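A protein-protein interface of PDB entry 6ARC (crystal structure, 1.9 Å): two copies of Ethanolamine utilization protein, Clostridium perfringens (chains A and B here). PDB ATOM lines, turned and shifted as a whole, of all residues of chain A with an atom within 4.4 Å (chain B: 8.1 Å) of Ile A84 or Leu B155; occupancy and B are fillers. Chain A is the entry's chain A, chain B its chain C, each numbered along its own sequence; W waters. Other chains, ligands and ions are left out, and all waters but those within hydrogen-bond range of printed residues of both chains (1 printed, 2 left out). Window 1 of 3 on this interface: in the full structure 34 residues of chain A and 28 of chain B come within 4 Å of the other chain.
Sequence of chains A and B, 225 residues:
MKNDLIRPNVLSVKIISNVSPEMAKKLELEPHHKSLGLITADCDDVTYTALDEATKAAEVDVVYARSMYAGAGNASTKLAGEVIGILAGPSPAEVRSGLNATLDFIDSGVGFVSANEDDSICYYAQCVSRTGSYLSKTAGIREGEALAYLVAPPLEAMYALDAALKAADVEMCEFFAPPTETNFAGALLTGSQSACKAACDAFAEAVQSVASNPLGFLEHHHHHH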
ATOM      1  N   SER A  12     -12.789 -11.829  19.096  1.00  0.00           N
ATOM      2  CA  SER A  12     -12.120 -12.114  17.831  1.00  0.00           C
ATOM      3  C   SER A  12     -11.254 -10.936  17.425  1.00  0.00           C
ATOM      4  O   SER A  12     -11.568  -9.785  17.734  1.00  0.00           O
ATOM      5  CB  SER A  12     -13.122 -12.418  16.721  1.00  0.00           C
ATOM      6  OG  SER A  12     -12.476 -12.954  15.580  1.00  0.00           O
ATOM      7  N   VAL A  13     -10.184 -11.240  16.694  1.00  0.00           N
ATOM      8  CA  VAL A  13      -9.273 -10.237  16.148  1.00  0.00           C
ATOM      9  C   VAL A  13      -8.765 -10.774  14.817  1.00  0.00           C
ATOM     10  O   VAL A  13      -8.360 -11.934  14.730  1.00  0.00           O
ATOM     11  CB  VAL A  13      -8.082  -9.961  17.101  1.00  0.00           C
ATOM     12  CG1 VAL A  13      -7.217  -8.856  16.530  1.00  0.00           C
ATOM     13  CG2 VAL A  13      -8.521  -9.595  18.478  1.00  0.00           C
ATOM     14  N   LYS A  14      -8.719  -9.912  13.805  1.00  0.00           N
ATOM     15  CA  LYS A  14      -8.207 -10.287  12.496  1.00  0.00           C
ATOM     16  C   LYS A  14      -7.573  -9.081  11.834  1.00  0.00           C
ATOM     17  O   LYS A  14      -7.973  -7.940  12.082  1.00  0.00           O
ATOM     18  CB  LYS A  14      -9.304 -10.827  11.590  1.00  0.00           C
ATOM     19  CG  LYS A  14      -9.806 -12.168  12.011  1.00  0.00           C
ATOM     20  CD  LYS A  14      -8.805 -13.262  11.696  1.00  0.00           C
ATOM     21  CE  LYS A  14      -9.105 -14.442  12.636  1.00  0.00           C
ATOM     22  NZ  LYS A  14      -8.264 -15.600  12.327  1.00  0.00           N
ATOM     23  N   LEU A  38      -9.472  -5.692  12.729  1.00  0.00           N
ATOM     24  CA  LEU A  38     -10.839  -5.908  13.193  1.00  0.00           C
ATOM     25  C   LEU A  38     -10.815  -6.521  14.578  1.00  0.00           C
ATOM     26  O   LEU A  38      -9.987  -7.396  14.849  1.00  0.00           O
ATOM     27  CB  LEU A  38     -11.567  -6.851  12.240  1.00  0.00           C
ATOM     28  CG  LEU A  38     -11.448  -6.651  10.730  1.00  0.00           C
ATOM     29  CD1 LEU A  38     -12.021  -7.896  10.024  1.00  0.00           C
ATOM     30  CD2 LEU A  38     -12.190  -5.436  10.280  1.00  0.00           C
ATOM     31  N   ILE A  39     -11.731  -6.074  15.448  1.00  0.00           N
ATOM     32  CA  ILE A  39     -11.835  -6.605  16.807  1.00  0.00           C
ATOM     33  C   ILE A  39     -13.295  -6.596  17.257  1.00  0.00           C
ATOM     34  O   ILE A  39     -14.061  -5.669  16.956  1.00  0.00           O
ATOM     35  CB  ILE A  39     -10.944  -5.809  17.794  1.00  0.00           C
ATOM     36  CG1 ILE A  39     -11.010  -6.441  19.166  1.00  0.00           C
ATOM     37  CG2 ILE A  39     -11.356  -4.364  17.887  1.00  0.00           C
ATOM     38  CD1 ILE A  39      -9.951  -5.913  20.152  1.00  0.00           C
ATOM     39  N   THR A  40     -13.692  -7.665  17.932  1.00  0.00           N
ATOM     40  CA  THR A  40     -14.955  -7.715  18.648  1.00  0.00           C
ATOM     41  C   THR A  40     -14.703  -8.139  20.071  1.00  0.00           C
ATOM     42  O   THR A  40     -13.721  -8.826  20.374  1.00  0.00           O
ATOM     43  CB  THR A  40     -15.970  -8.680  18.040  1.00  0.00           C
ATOM     44  OG1 THR A  40     -15.482 -10.025  18.125  1.00  0.00           O
ATOM     45  CG2 THR A  40     -16.255  -8.297  16.581  1.00  0.00           C
ATOM     46  N   TYR A  64     -14.127   2.565  12.239  1.00  0.00           N
ATOM     47  CA  TYR A  64     -15.441   1.958  12.409  1.00  0.00           C
ATOM     48  C   TYR A  64     -15.565   1.586  13.863  1.00  0.00           C
ATOM     49  O   TYR A  64     -14.638   1.027  14.451  1.00  0.00           O
ATOM     50  CB  TYR A  64     -15.627   0.703  11.550  1.00  0.00           C
ATOM     51  CG  TYR A  64     -17.079   0.353  11.284  1.00  0.00           C
ATOM     52  CD1 TYR A  64     -17.752   0.906  10.217  1.00  0.00           C
ATOM     53  CD2 TYR A  64     -17.766  -0.527  12.106  1.00  0.00           C
ATOM     54  CE1 TYR A  64     -19.088   0.599   9.968  1.00  0.00           C
ATOM     55  CE2 TYR A  64     -19.077  -0.835  11.859  1.00  0.00           C
ATOM     56  CZ  TYR A  64     -19.732  -0.279  10.786  1.00  0.00           C
ATOM     57  OH  TYR A  64     -21.054  -0.582  10.558  1.00  0.00           O
ATOM     58  N   ALA A  65     -16.719   1.878  14.439  1.00  0.00           N
ATOM     59  CA  ALA A  65     -16.933   1.548  15.840  1.00  0.00           C
ATOM     60  C   ALA A  65     -18.438   1.541  16.096  1.00  0.00           C
ATOM     61  O   ALA A  65     -19.051   2.607  16.179  1.00  0.00           O
ATOM     62  CB  ALA A  65     -16.201   2.556  16.720  1.00  0.00           C
ATOM     63  N   ARG A  66     -19.029   0.351  16.228  1.00  0.00           N
ATOM     64  CA  ARG A  66     -20.471   0.256  16.435  1.00  0.00           C
ATOM     65  C   ARG A  66     -20.788  -0.788  17.489  1.00  0.00           C
ATOM     66  O   ARG A  66     -20.105  -1.806  17.593  1.00  0.00           O
ATOM     67  CB  ARG A  66     -21.212  -0.115  15.134  1.00  0.00           C
ATOM     68  CG  ARG A  66     -21.146   0.925  14.018  1.00  0.00           C
ATOM     69  CD  ARG A  66     -21.915   2.182  14.344  1.00  0.00           C
ATOM     70  NE  ARG A  66     -23.282   1.918  14.836  1.00  0.00           N
ATOM     71  CZ  ARG A  66     -24.298   1.530  14.079  1.00  0.00           C
ATOM     72  NH1 ARG A  66     -24.122   1.355  12.777  1.00  0.00           N
ATOM     73  NH2 ARG A  66     -25.497   1.315  14.629  1.00  0.00           N
ATOM     74  N   MET A  68     -23.707  -3.455  19.376  1.00  0.00           N
ATOM     75  CA  MET A  68     -24.714  -4.430  18.972  1.00  0.00           C
ATOM     76  C   MET A  68     -25.997  -4.243  19.767  1.00  0.00           C
ATOM     77  O   MET A  68     -25.972  -3.919  20.962  1.00  0.00           O
ATOM     78  CB  MET A  68     -24.198  -5.853  19.162  1.00  0.00           C
ATOM     79  CG  MET A  68     -22.877  -6.130  18.442  1.00  0.00           C
ATOM     80  SD  MET A  68     -23.056  -6.135  16.649  1.00  0.00           S
ATOM     81  CE  MET A  68     -22.069  -4.754  16.160  1.00  0.00           C
ATOM     82  N   VAL A  83     -19.662  -5.292  20.380  1.00  0.00           N
ATOM     83  CA  VAL A  83     -18.949  -4.217  19.724  1.00  0.00           C
ATOM     84  C   VAL A  83     -18.135  -4.777  18.564  1.00  0.00           C
ATOM     85  O   VAL A  83     -17.607  -5.896  18.628  1.00  0.00           O
ATOM     86  CB  VAL A  83     -18.050  -3.464  20.727  1.00  0.00           C
ATOM     87  CG1 VAL A  83     -16.969  -4.389  21.293  1.00  0.00           C
ATOM     88  CG2 VAL A  83     -17.430  -2.283  20.061  1.00  0.00           C
ATOM     89  N   ILE A  84     -18.065  -3.993  17.495  1.00  0.00           N
ATOM     90  CA  ILE A  84     -17.073  -4.190  16.454  1.00  0.00           C
ATOM     91  C   ILE A  84     -16.300  -2.888  16.305  1.00  0.00           C
ATOM     92  O   ILE A  84     -16.892  -1.802  16.202  1.00  0.00           O
ATOM     93  CB  ILE A  84     -17.683  -4.633  15.107  1.00  0.00           C
ATOM     94  CG1 ILE A  84     -16.526  -4.808  14.095  1.00  0.00           C
ATOM     95  CG2 ILE A  84     -18.744  -3.647  14.621  1.00  0.00           C
ATOM     96  CD1 ILE A  84     -16.873  -5.505  12.888  1.00  0.00           C
ATOM     97  N   GLY A  85     -14.980  -3.005  16.288  1.00  0.00           N
ATOM     98  CA  GLY A  85     -14.124  -1.880  15.995  1.00  0.00           C
ATOM     99  C   GLY A  85     -13.172  -2.228  14.866  1.00  0.00           C
ATOM    100  O   GLY A  85     -12.784  -3.380  14.691  1.00  0.00           O
ATOM    101  N   ALA B 152     -22.996 -12.730   7.560  1.00  0.00           N
ATOM    102  CA  ALA B 152     -22.332 -13.397   8.674  1.00  0.00           C
ATOM    103  C   ALA B 152     -22.301 -12.426   9.843  1.00  0.00           C
ATOM    104  O   ALA B 152     -22.739 -11.271   9.718  1.00  0.00           O
ATOM    105  CB  ALA B 152     -20.915 -13.851   8.305  1.00  0.00           C
ATOM    106  N   PRO B 153     -21.858 -12.869  11.013  1.00  0.00           N
ATOM    107  CA  PRO B 153     -21.751 -11.937  12.126  1.00  0.00           C
ATOM    108  C   PRO B 153     -20.689 -10.898  11.831  1.00  0.00           C
ATOM    109  O   PRO B 153     -19.889 -11.068  10.902  1.00  0.00           O
ATOM    110  CB  PRO B 153     -21.372 -12.828  13.321  1.00  0.00           C
ATOM    111  CG  PRO B 153     -21.871 -14.191  12.942  1.00  0.00           C
ATOM    112  CD  PRO B 153     -21.677 -14.271  11.440  1.00  0.00           C
ATOM    113  N   PRO B 154     -20.653  -9.817  12.598  1.00  0.00           N
ATOM    114  CA  PRO B 154     -19.955  -8.603  12.131  1.00  0.00           C
ATOM    115  C   PRO B 154     -18.506  -8.783  11.700  1.00  0.00           C
ATOM    116  O   PRO B 154     -18.149  -8.364  10.595  1.00  0.00           O
ATOM    117  CB  PRO B 154     -20.100  -7.669  13.329  1.00  0.00           C
ATOM    118  CG  PRO B 154     -21.412  -8.072  13.947  1.00  0.00           C
ATOM    119  CD  PRO B 154     -21.473  -9.565  13.803  1.00  0.00           C
ATOM    120  N   LEU B 155     -17.642  -9.361  12.538  1.00  0.00           N
ATOM    121  CA  LEU B 155     -16.234  -9.438  12.153  1.00  0.00           C
ATOM    122  C   LEU B 155     -16.040 -10.434  11.029  1.00  0.00           C
ATOM    123  O   LEU B 155     -15.353 -10.144  10.039  1.00  0.00           O
ATOM    124  CB  LEU B 155     -15.356  -9.804  13.354  1.00  0.00           C
ATOM    125  CG  LEU B 155     -13.852  -9.875  13.033  1.00  0.00           C
ATOM    126  CD1 LEU B 155     -13.054  -9.372  14.245  1.00  0.00           C
ATOM    127  CD2 LEU B 155     -13.444 -11.289  12.650  1.00  0.00           C
ATOM    128  N   GLU B 156     -16.645 -11.613  11.163  1.00  0.00           N
ATOM    129  CA  GLU B 156     -16.584 -12.615  10.107  1.00  0.00           C
ATOM    130  C   GLU B 156     -17.000 -12.019   8.779  1.00  0.00           C
ATOM    131  O   GLU B 156     -16.381 -12.285   7.741  1.00  0.00           O
ATOM    132  CB  GLU B 156     -17.499 -13.794  10.436  1.00  0.00           C
ATOM    133  CG  GLU B 156     -17.161 -14.553  11.705  1.00  0.00           C
ATOM    134  CD  GLU B 156     -17.912 -14.033  12.935  1.00  0.00           C
ATOM    135  OE1 GLU B 156     -17.846 -12.807  13.218  1.00  0.00           O
ATOM    136  OE2 GLU B 156     -18.574 -14.853  13.604  1.00  0.00           O
ATOM    137  N   ALA B 157     -18.082 -11.240   8.788  1.00  0.00           N
ATOM    138  CA  ALA B 157     -18.609 -10.701   7.539  1.00  0.00           C
ATOM    139  C   ALA B 157     -17.638  -9.715   6.906  1.00  0.00           C
ATOM    140  O   ALA B 157     -17.446  -9.740   5.691  1.00  0.00           O
ATOM    141  CB  ALA B 157     -19.966 -10.051   7.782  1.00  0.00           C
ATOM    142  N   MET B 158     -17.043  -8.805   7.693  1.00  0.00           N
ATOM    143  CA  MET B 158     -16.111  -7.843   7.105  1.00  0.00           C
ATOM    144  C   MET B 158     -14.893  -8.558   6.531  1.00  0.00           C
ATOM    145  O   MET B 158     -14.437  -8.268   5.418  1.00  0.00           O
ATOM    146  CB  MET B 158     -15.690  -6.814   8.159  1.00  0.00           C
ATOM    147  CG  MET B 158     -16.857  -6.028   8.707  1.00  0.00           C
ATOM    148  SD  MET B 158     -17.708  -5.040   7.454  1.00  0.00           S
ATOM    149  CE  MET B 158     -16.459  -3.789   7.158  1.00  0.00           C
ATOM    150  N   TYR B 159     -14.364  -9.514   7.281  1.00  0.00           N
ATOM    151  CA  TYR B 159     -13.211 -10.280   6.830  1.00  0.00           C
ATOM    152  C   TYR B 159     -13.541 -11.074   5.571  1.00  0.00           C
ATOM    153  O   TYR B 159     -12.737 -11.154   4.632  1.00  0.00           O
ATOM    154  CB  TYR B 159     -12.796 -11.214   7.959  1.00  0.00           C
ATOM    155  CG  TYR B 159     -11.551 -12.024   7.705  1.00  0.00           C
ATOM    156  CD1 TYR B 159     -10.295 -11.469   7.957  1.00  0.00           C
ATOM    157  CD2 TYR B 159     -11.613 -13.332   7.237  1.00  0.00           C
ATOM    158  CE1 TYR B 159      -9.141 -12.188   7.755  1.00  0.00           C
ATOM    159  CE2 TYR B 159     -10.459 -14.058   7.012  1.00  0.00           C
ATOM    160  CZ  TYR B 159      -9.215 -13.473   7.283  1.00  0.00           C
ATOM    161  OH  TYR B 159      -8.023 -14.143   7.092  1.00  0.00           O
ATOM    162  N   ALA B 160     -14.686 -11.743   5.575  1.00  0.00           N
ATOM    163  CA  ALA B 160     -15.040 -12.631   4.474  1.00  0.00           C
ATOM    164  C   ALA B 160     -15.533 -11.873   3.250  1.00  0.00           C
ATOM    165  O   ALA B 160     -15.370 -12.370   2.131  1.00  0.00           O
ATOM    166  CB  ALA B 160     -16.076 -13.645   4.958  1.00  0.00           C
ATOM    167  N   LEU B 161     -16.127 -10.685   3.432  1.00  0.00           N
ATOM    168  CA  LEU B 161     -16.477  -9.850   2.287  1.00  0.00           C
ATOM    169  C   LEU B 161     -15.225  -9.446   1.525  1.00  0.00           C
ATOM    170  O   LEU B 161     -15.193  -9.480   0.287  1.00  0.00           O
ATOM    171  CB  LEU B 161     -17.256  -8.608   2.731  1.00  0.00           C
ATOM    172  CG  LEU B 161     -18.741  -8.787   3.047  1.00  0.00           C
ATOM    173  CD1 LEU B 161     -19.330  -7.427   3.430  1.00  0.00           C
ATOM    174  CD2 LEU B 161     -19.542  -9.415   1.876  1.00  0.00           C
ATOM    175  N   ASP B 162     -14.170  -9.074   2.251  1.00  0.00           N
ATOM    176  CA  ASP B 162     -12.909  -8.765   1.595  1.00  0.00           C
ATOM    177  C   ASP B 162     -12.391  -9.977   0.816  1.00  0.00           C
ATOM    178  O   ASP B 162     -11.983  -9.848  -0.341  1.00  0.00           O
ATOM    179  CB  ASP B 162     -11.895  -8.284   2.635  1.00  0.00           C
ATOM    180  CG  ASP B 162     -10.592  -7.816   1.998  1.00  0.00           C
ATOM    181  OD1 ASP B 162     -10.606  -6.714   1.391  1.00  0.00           O
ATOM    182  OD2 ASP B 162      -9.595  -8.563   2.078  1.00  0.00           O
ATOM    183  N   ALA B 177     -24.181  -2.821   6.755  1.00  0.00           N
ATOM    184  CA  ALA B 177     -23.136  -2.435   7.705  1.00  0.00           C
ATOM    185  C   ALA B 177     -23.460  -2.981   9.099  1.00  0.00           C
ATOM    186  O   ALA B 177     -24.612  -2.925   9.545  1.00  0.00           O
ATOM    187  CB  ALA B 177     -22.994  -0.911   7.772  1.00  0.00           C
ATOM    188  N   PRO B 178     -22.485  -3.513   9.818  1.00  0.00           N
ATOM    189  CA  PRO B 178     -22.794  -4.068  11.147  1.00  0.00           C
ATOM    190  C   PRO B 178     -23.065  -2.968  12.159  1.00  0.00           C
ATOM    191  O   PRO B 178     -22.305  -1.998  12.232  1.00  0.00           O
ATOM    192  CB  PRO B 178     -21.538  -4.864  11.508  1.00  0.00           C
ATOM    193  CG  PRO B 178     -20.444  -4.264  10.704  1.00  0.00           C
ATOM    194  CD  PRO B 178     -21.079  -3.727   9.435  1.00  0.00           C
ATOM    195  N   PRO B 179     -24.115  -3.109  13.004  1.00  0.00           N
ATOM    196  CA  PRO B 179     -25.083  -4.215  13.035  1.00  0.00           C
ATOM    197  C   PRO B 179     -26.293  -3.963  12.158  1.00  0.00           C
ATOM    198  O   PRO B 179     -26.756  -2.847  12.106  1.00  0.00           O
ATOM    199  CB  PRO B 179     -25.518  -4.240  14.509  1.00  0.00           C
ATOM    200  CG  PRO B 179     -25.500  -2.823  14.888  1.00  0.00           C
ATOM    201  CD  PRO B 179     -24.300  -2.225  14.176  1.00  0.00           C
ATOM    202  N   ASN B 183     -27.998  -7.987  14.280  1.00  0.00           N
ATOM    203  CA  ASN B 183     -26.578  -7.983  14.649  1.00  0.00           C
ATOM    204  C   ASN B 183     -25.741  -8.868  13.715  1.00  0.00           C
ATOM    205  O   ASN B 183     -24.773  -9.503  14.130  1.00  0.00           O
ATOM    206  CB  ASN B 183     -26.389  -8.395  16.124  1.00  0.00           C
ATOM    207  CG  ASN B 183     -27.057  -7.430  17.085  1.00  0.00           C
ATOM    208  OD1 ASN B 183     -26.996  -6.217  16.907  1.00  0.00           O
ATOM    209  ND2 ASN B 183     -27.779  -7.979  18.074  1.00  0.00           N
ATOM    210  N   PHE B 184     -26.125  -8.916  12.450  1.00  0.00           N
ATOM    211  CA  PHE B 184     -25.324  -9.498  11.391  1.00  0.00           C
ATOM    212  C   PHE B 184     -24.830  -8.374  10.486  1.00  0.00           C
ATOM    213  O   PHE B 184     -25.018  -7.171  10.772  1.00  0.00           O
ATOM    214  CB  PHE B 184     -26.143 -10.545  10.635  1.00  0.00           C
ATOM    215  CG  PHE B 184     -26.227 -11.877  11.338  1.00  0.00           C
ATOM    216  CD1 PHE B 184     -27.058 -12.056  12.426  1.00  0.00           C
ATOM    217  CD2 PHE B 184     -25.462 -12.942  10.901  1.00  0.00           C
ATOM    218  CE1 PHE B 184     -27.132 -13.291  13.078  1.00  0.00           C
ATOM    219  CE2 PHE B 184     -25.513 -14.168  11.534  1.00  0.00           C
ATOM    220  CZ  PHE B 184     -26.367 -14.354  12.638  1.00  0.00           C
ATOM    221  N   ALA B 185     -24.164  -8.766   9.405  1.00  0.00           N
ATOM    222  CA  ALA B 185     -23.605  -7.852   8.424  1.00  0.00           C
ATOM    223  C   ALA B 185     -23.390  -8.658   7.155  1.00  0.00           C
ATOM    224  O   ALA B 185     -23.438  -9.888   7.169  1.00  0.00           O
ATOM    225  CB  ALA B 185     -22.288  -7.237   8.895  1.00  0.00           C
ATOM    226  N   PHE B 203     -16.427 -16.516   0.431  1.00  0.00           N
ATOM    227  CA  PHE B 203     -17.026 -15.990   1.654  1.00  0.00           C
ATOM    228  C   PHE B 203     -17.195 -17.091   2.702  1.00  0.00           C
ATOM    229  O   PHE B 203     -16.802 -16.938   3.870  1.00  0.00           O
ATOM    230  CB  PHE B 203     -18.352 -15.344   1.305  1.00  0.00           C
ATOM    231  CG  PHE B 203     -19.026 -14.667   2.454  1.00  0.00           C
ATOM    232  CD1 PHE B 203     -18.673 -13.392   2.823  1.00  0.00           C
ATOM    233  CD2 PHE B 203     -20.046 -15.299   3.134  1.00  0.00           C
ATOM    234  CE1 PHE B 203     -19.334 -12.745   3.883  1.00  0.00           C
ATOM    235  CE2 PHE B 203     -20.711 -14.662   4.193  1.00  0.00           C
ATOM    236  CZ  PHE B 203     -20.357 -13.391   4.553  1.00  0.00           C
ATOM    237  N   ALA B 206     -13.840 -18.160   4.183  1.00  0.00           N
ATOM    238  CA  ALA B 206     -13.282 -17.135   5.059  1.00  0.00           C
ATOM    239  C   ALA B 206     -14.030 -17.072   6.392  1.00  0.00           C
ATOM    240  O   ALA B 206     -13.407 -16.986   7.456  1.00  0.00           O
ATOM    241  CB  ALA B 206     -13.326 -15.772   4.343  1.00  0.00           C
ATOM    242  N   VAL B 207     -15.359 -17.152   6.368  1.00  0.00           N
ATOM    243  CA  VAL B 207     -16.102 -17.186   7.628  1.00  0.00           C
ATOM    244  C   VAL B 207     -15.654 -18.379   8.457  1.00  0.00           C
ATOM    245  O   VAL B 207     -15.432 -18.273   9.667  1.00  0.00           O
ATOM    246  CB  VAL B 207     -17.623 -17.237   7.390  1.00  0.00           C
ATOM    247  CG1 VAL B 207     -18.300 -17.445   8.716  1.00  0.00           C
ATOM    248  CG2 VAL B 207     -18.128 -15.945   6.758  1.00  0.00           C
ATOM    249  N   VAL B 210     -12.371 -17.873  10.236  1.00  0.00           N
ATOM    250  CA  VAL B 210     -12.468 -17.081  11.466  1.00  0.00           C
ATOM    251  C   VAL B 210     -13.051 -17.929  12.594  1.00  0.00           C
ATOM    252  O   VAL B 210     -12.549 -17.927  13.731  1.00  0.00           O
ATOM    253  CB  VAL B 210     -13.299 -15.806  11.231  1.00  0.00           C
ATOM    254  CG1 VAL B 210     -13.410 -14.975  12.523  1.00  0.00           C
ATOM    255  CG2 VAL B 210     -12.678 -14.978  10.153  1.00  0.00           C
ATOM    256  N   ALA B 211     -14.123 -18.666  12.300  1.00  0.00           N
ATOM    257  CA  ALA B 211     -14.728 -19.525  13.315  1.00  0.00           C
ATOM    258  C   ALA B 211     -13.714 -20.529  13.864  1.00  0.00           C
ATOM    259  O   ALA B 211     -13.685 -20.794  15.072  1.00  0.00           O
ATOM    260  CB  ALA B 211     -15.960 -20.248  12.735  1.00  0.00           C
ATOM    261  N   ASN B 213     -10.433 -20.175  14.055  1.00  0.00           N
ATOM    262  CA  ASN B 213      -9.329 -19.516  14.760  1.00  0.00           C
ATOM    263  C   ASN B 213      -9.661 -18.044  14.991  1.00  0.00           C
ATOM    264  O   ASN B 213      -9.086 -17.145  14.359  1.00  0.00           O
ATOM    265  CB  ASN B 213      -8.037 -19.674  13.972  1.00  0.00           C
ATOM    266  CG  ASN B 213      -6.849 -19.068  14.696  1.00  0.00           C
ATOM    267  OD1 ASN B 213      -6.096 -18.300  14.116  1.00  0.00           O
ATOM    268  ND2 ASN B 213      -6.697 -19.396  15.970  1.00  0.00           N
ATOM    269  N   PRO B 214     -10.610 -17.761  15.881  1.00  0.00           N
ATOM    270  CA  PRO B 214     -11.106 -16.368  16.002  1.00  0.00           C
ATOM    271  C   PRO B 214     -10.089 -15.357  16.508  1.00  0.00           C
ATOM    272  O   PRO B 214     -10.202 -14.172  16.171  1.00  0.00           O
ATOM    273  CB  PRO B 214     -12.297 -16.496  16.973  1.00  0.00           C
ATOM    274  CG  PRO B 214     -12.192 -17.844  17.567  1.00  0.00           C
ATOM    275  CD  PRO B 214     -11.434 -18.717  16.638  1.00  0.00           C
ATOM    276  N   LEU B 215      -9.130 -15.762  17.339  1.00  0.00           N
ATOM    277  CA  LEU B 215      -8.208 -14.813  17.962  1.00  0.00           C
ATOM    278  C   LEU B 215      -6.813 -14.823  17.348  1.00  0.00           C
ATOM    279  O   LEU B 215      -5.982 -13.990  17.723  1.00  0.00           O
ATOM    280  CB  LEU B 215      -8.120 -15.119  19.457  1.00  0.00           C
ATOM    281  CG  LEU B 215      -9.412 -14.803  20.230  1.00  0.00           C
ATOM    282  CD1 LEU B 215      -9.460 -15.381  21.633  1.00  0.00           C
ATOM    283  CD2 LEU B 215      -9.626 -13.317  20.320  1.00  0.00           C
HETATM  284  O   HOH W   1      -8.965 -16.425   9.347  1.00  0.00           O
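O of Ile A39 lies within hydrogen-bond range of N of Gly A85 (2.9 Å).
The backbone NH (N) of Leu A38 lies within hydrogen-bond range of the backbone carbonyl oxygen (O) of Lys A14, 2.8 Å away.
O of Ser A12 lies within hydrogen-bond range of N of Thr A40, 3.0 Å away.
O of Arg A66 is in hydrogen-bond range of N of Ile A84 (3.0 Å).
O of Asn B213 lies within hydrogen-bond range of NZ of Lys A14, at 2.7 Å.
The backbone NH (N) of Val A13 sits at hydrogen-bond distance from the backbone carbonyl oxygen (O) of Pro B214 (3.0 Å).
The backbone carbonyl oxygen (O) of Pro B214 sits at hydrogen-bond distance from the side-chain hydroxyl (OG) of Ser A12, at 2.6 Å.
The backbone carbonyl oxygen (O) of Pro B178 lies within hydrogen-bond range of the side-chain hydroxyl (OH) of Tyr A64 (2.5 Å).
Water W1 bridges NZ of Lys A14 and OH of Tyr B159.
Hydrophobic or aromatic side chains of chain B within 4 Å of the printed part of chain A: Pro B154, Leu B155, Tyr B159, Ala B177, Pro B178, Pro B179, Val B210, Pro B214 and Leu B215.
Printed residues of chain A that touch a printed residue of chain B: Ser A12, Val A13, Lys A14, Leu A38, Ile A39, Thr A40, Tyr A64, Arg A66, Met A68 and Ile A84.
Along chain A the printed residues that touch a printed residue of chain B span positions 12 to 84.
Among the printed residues, 22 pairs touch across the chains.
Among the printed residues, pairs that only touch across the chains: Ser A12 with Leu B155, Ser A12 with Val B210, Ser A12 with Leu B215, Lys A14 with Leu B155, Lys A14 with Tyr B159, Lys A14 with Pro B214, Leu A38 with Leu B155, Leu A38 with Tyr B159, Ile A39 with Leu B155, Thr A40 with Leu B155, Tyr A64 with Ala B177, Arg A66 with Pro B178, Arg A66 with Pro B179, Met A68 with Pro B154, Met A68 with Pro B179, Met A68 with Asn B183, Ile A84 with Pro B154 and Ile A84 with Leu B155.
No position is printed for both chains.
Printed residues of chain B within 4 Å of Ile A84: Pro B154 and Leu B155.
Of the printed residues of chain A, Leu B155 touches Ser A12 (3.5 Å), Lys A14 (3.8 Å), Leu A38 (3.5 Å), Ile A39 (3.8 Å), Thr A40 (3.7 Å) and Ile A84 (3.9 Å).
No residue of chain B comes within 4 Å of Val A83.
Printed residues of chain B within 4 Å of Thr A40: Leu B155 (3.7 Å).
Printed residues of chain A within 4 Å of Tyr B159: Lys A14 (3.8 Å) and Leu A38 (3.95 Å).
Of the printed residues of chain A, Pro B178 touches Tyr A64 (2.5 Å) and Arg A66 (3.6 Å).
Printed residues of chain B within 4 Å of Val A13: Pro B214 (3.0 Å).
Of the printed residues of chain A, Asn B183 touches Met A68 (3.6 Å).
The nearest printed residue of chain B that does not touch Val A13 is Leu B215 (4.2 Å).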
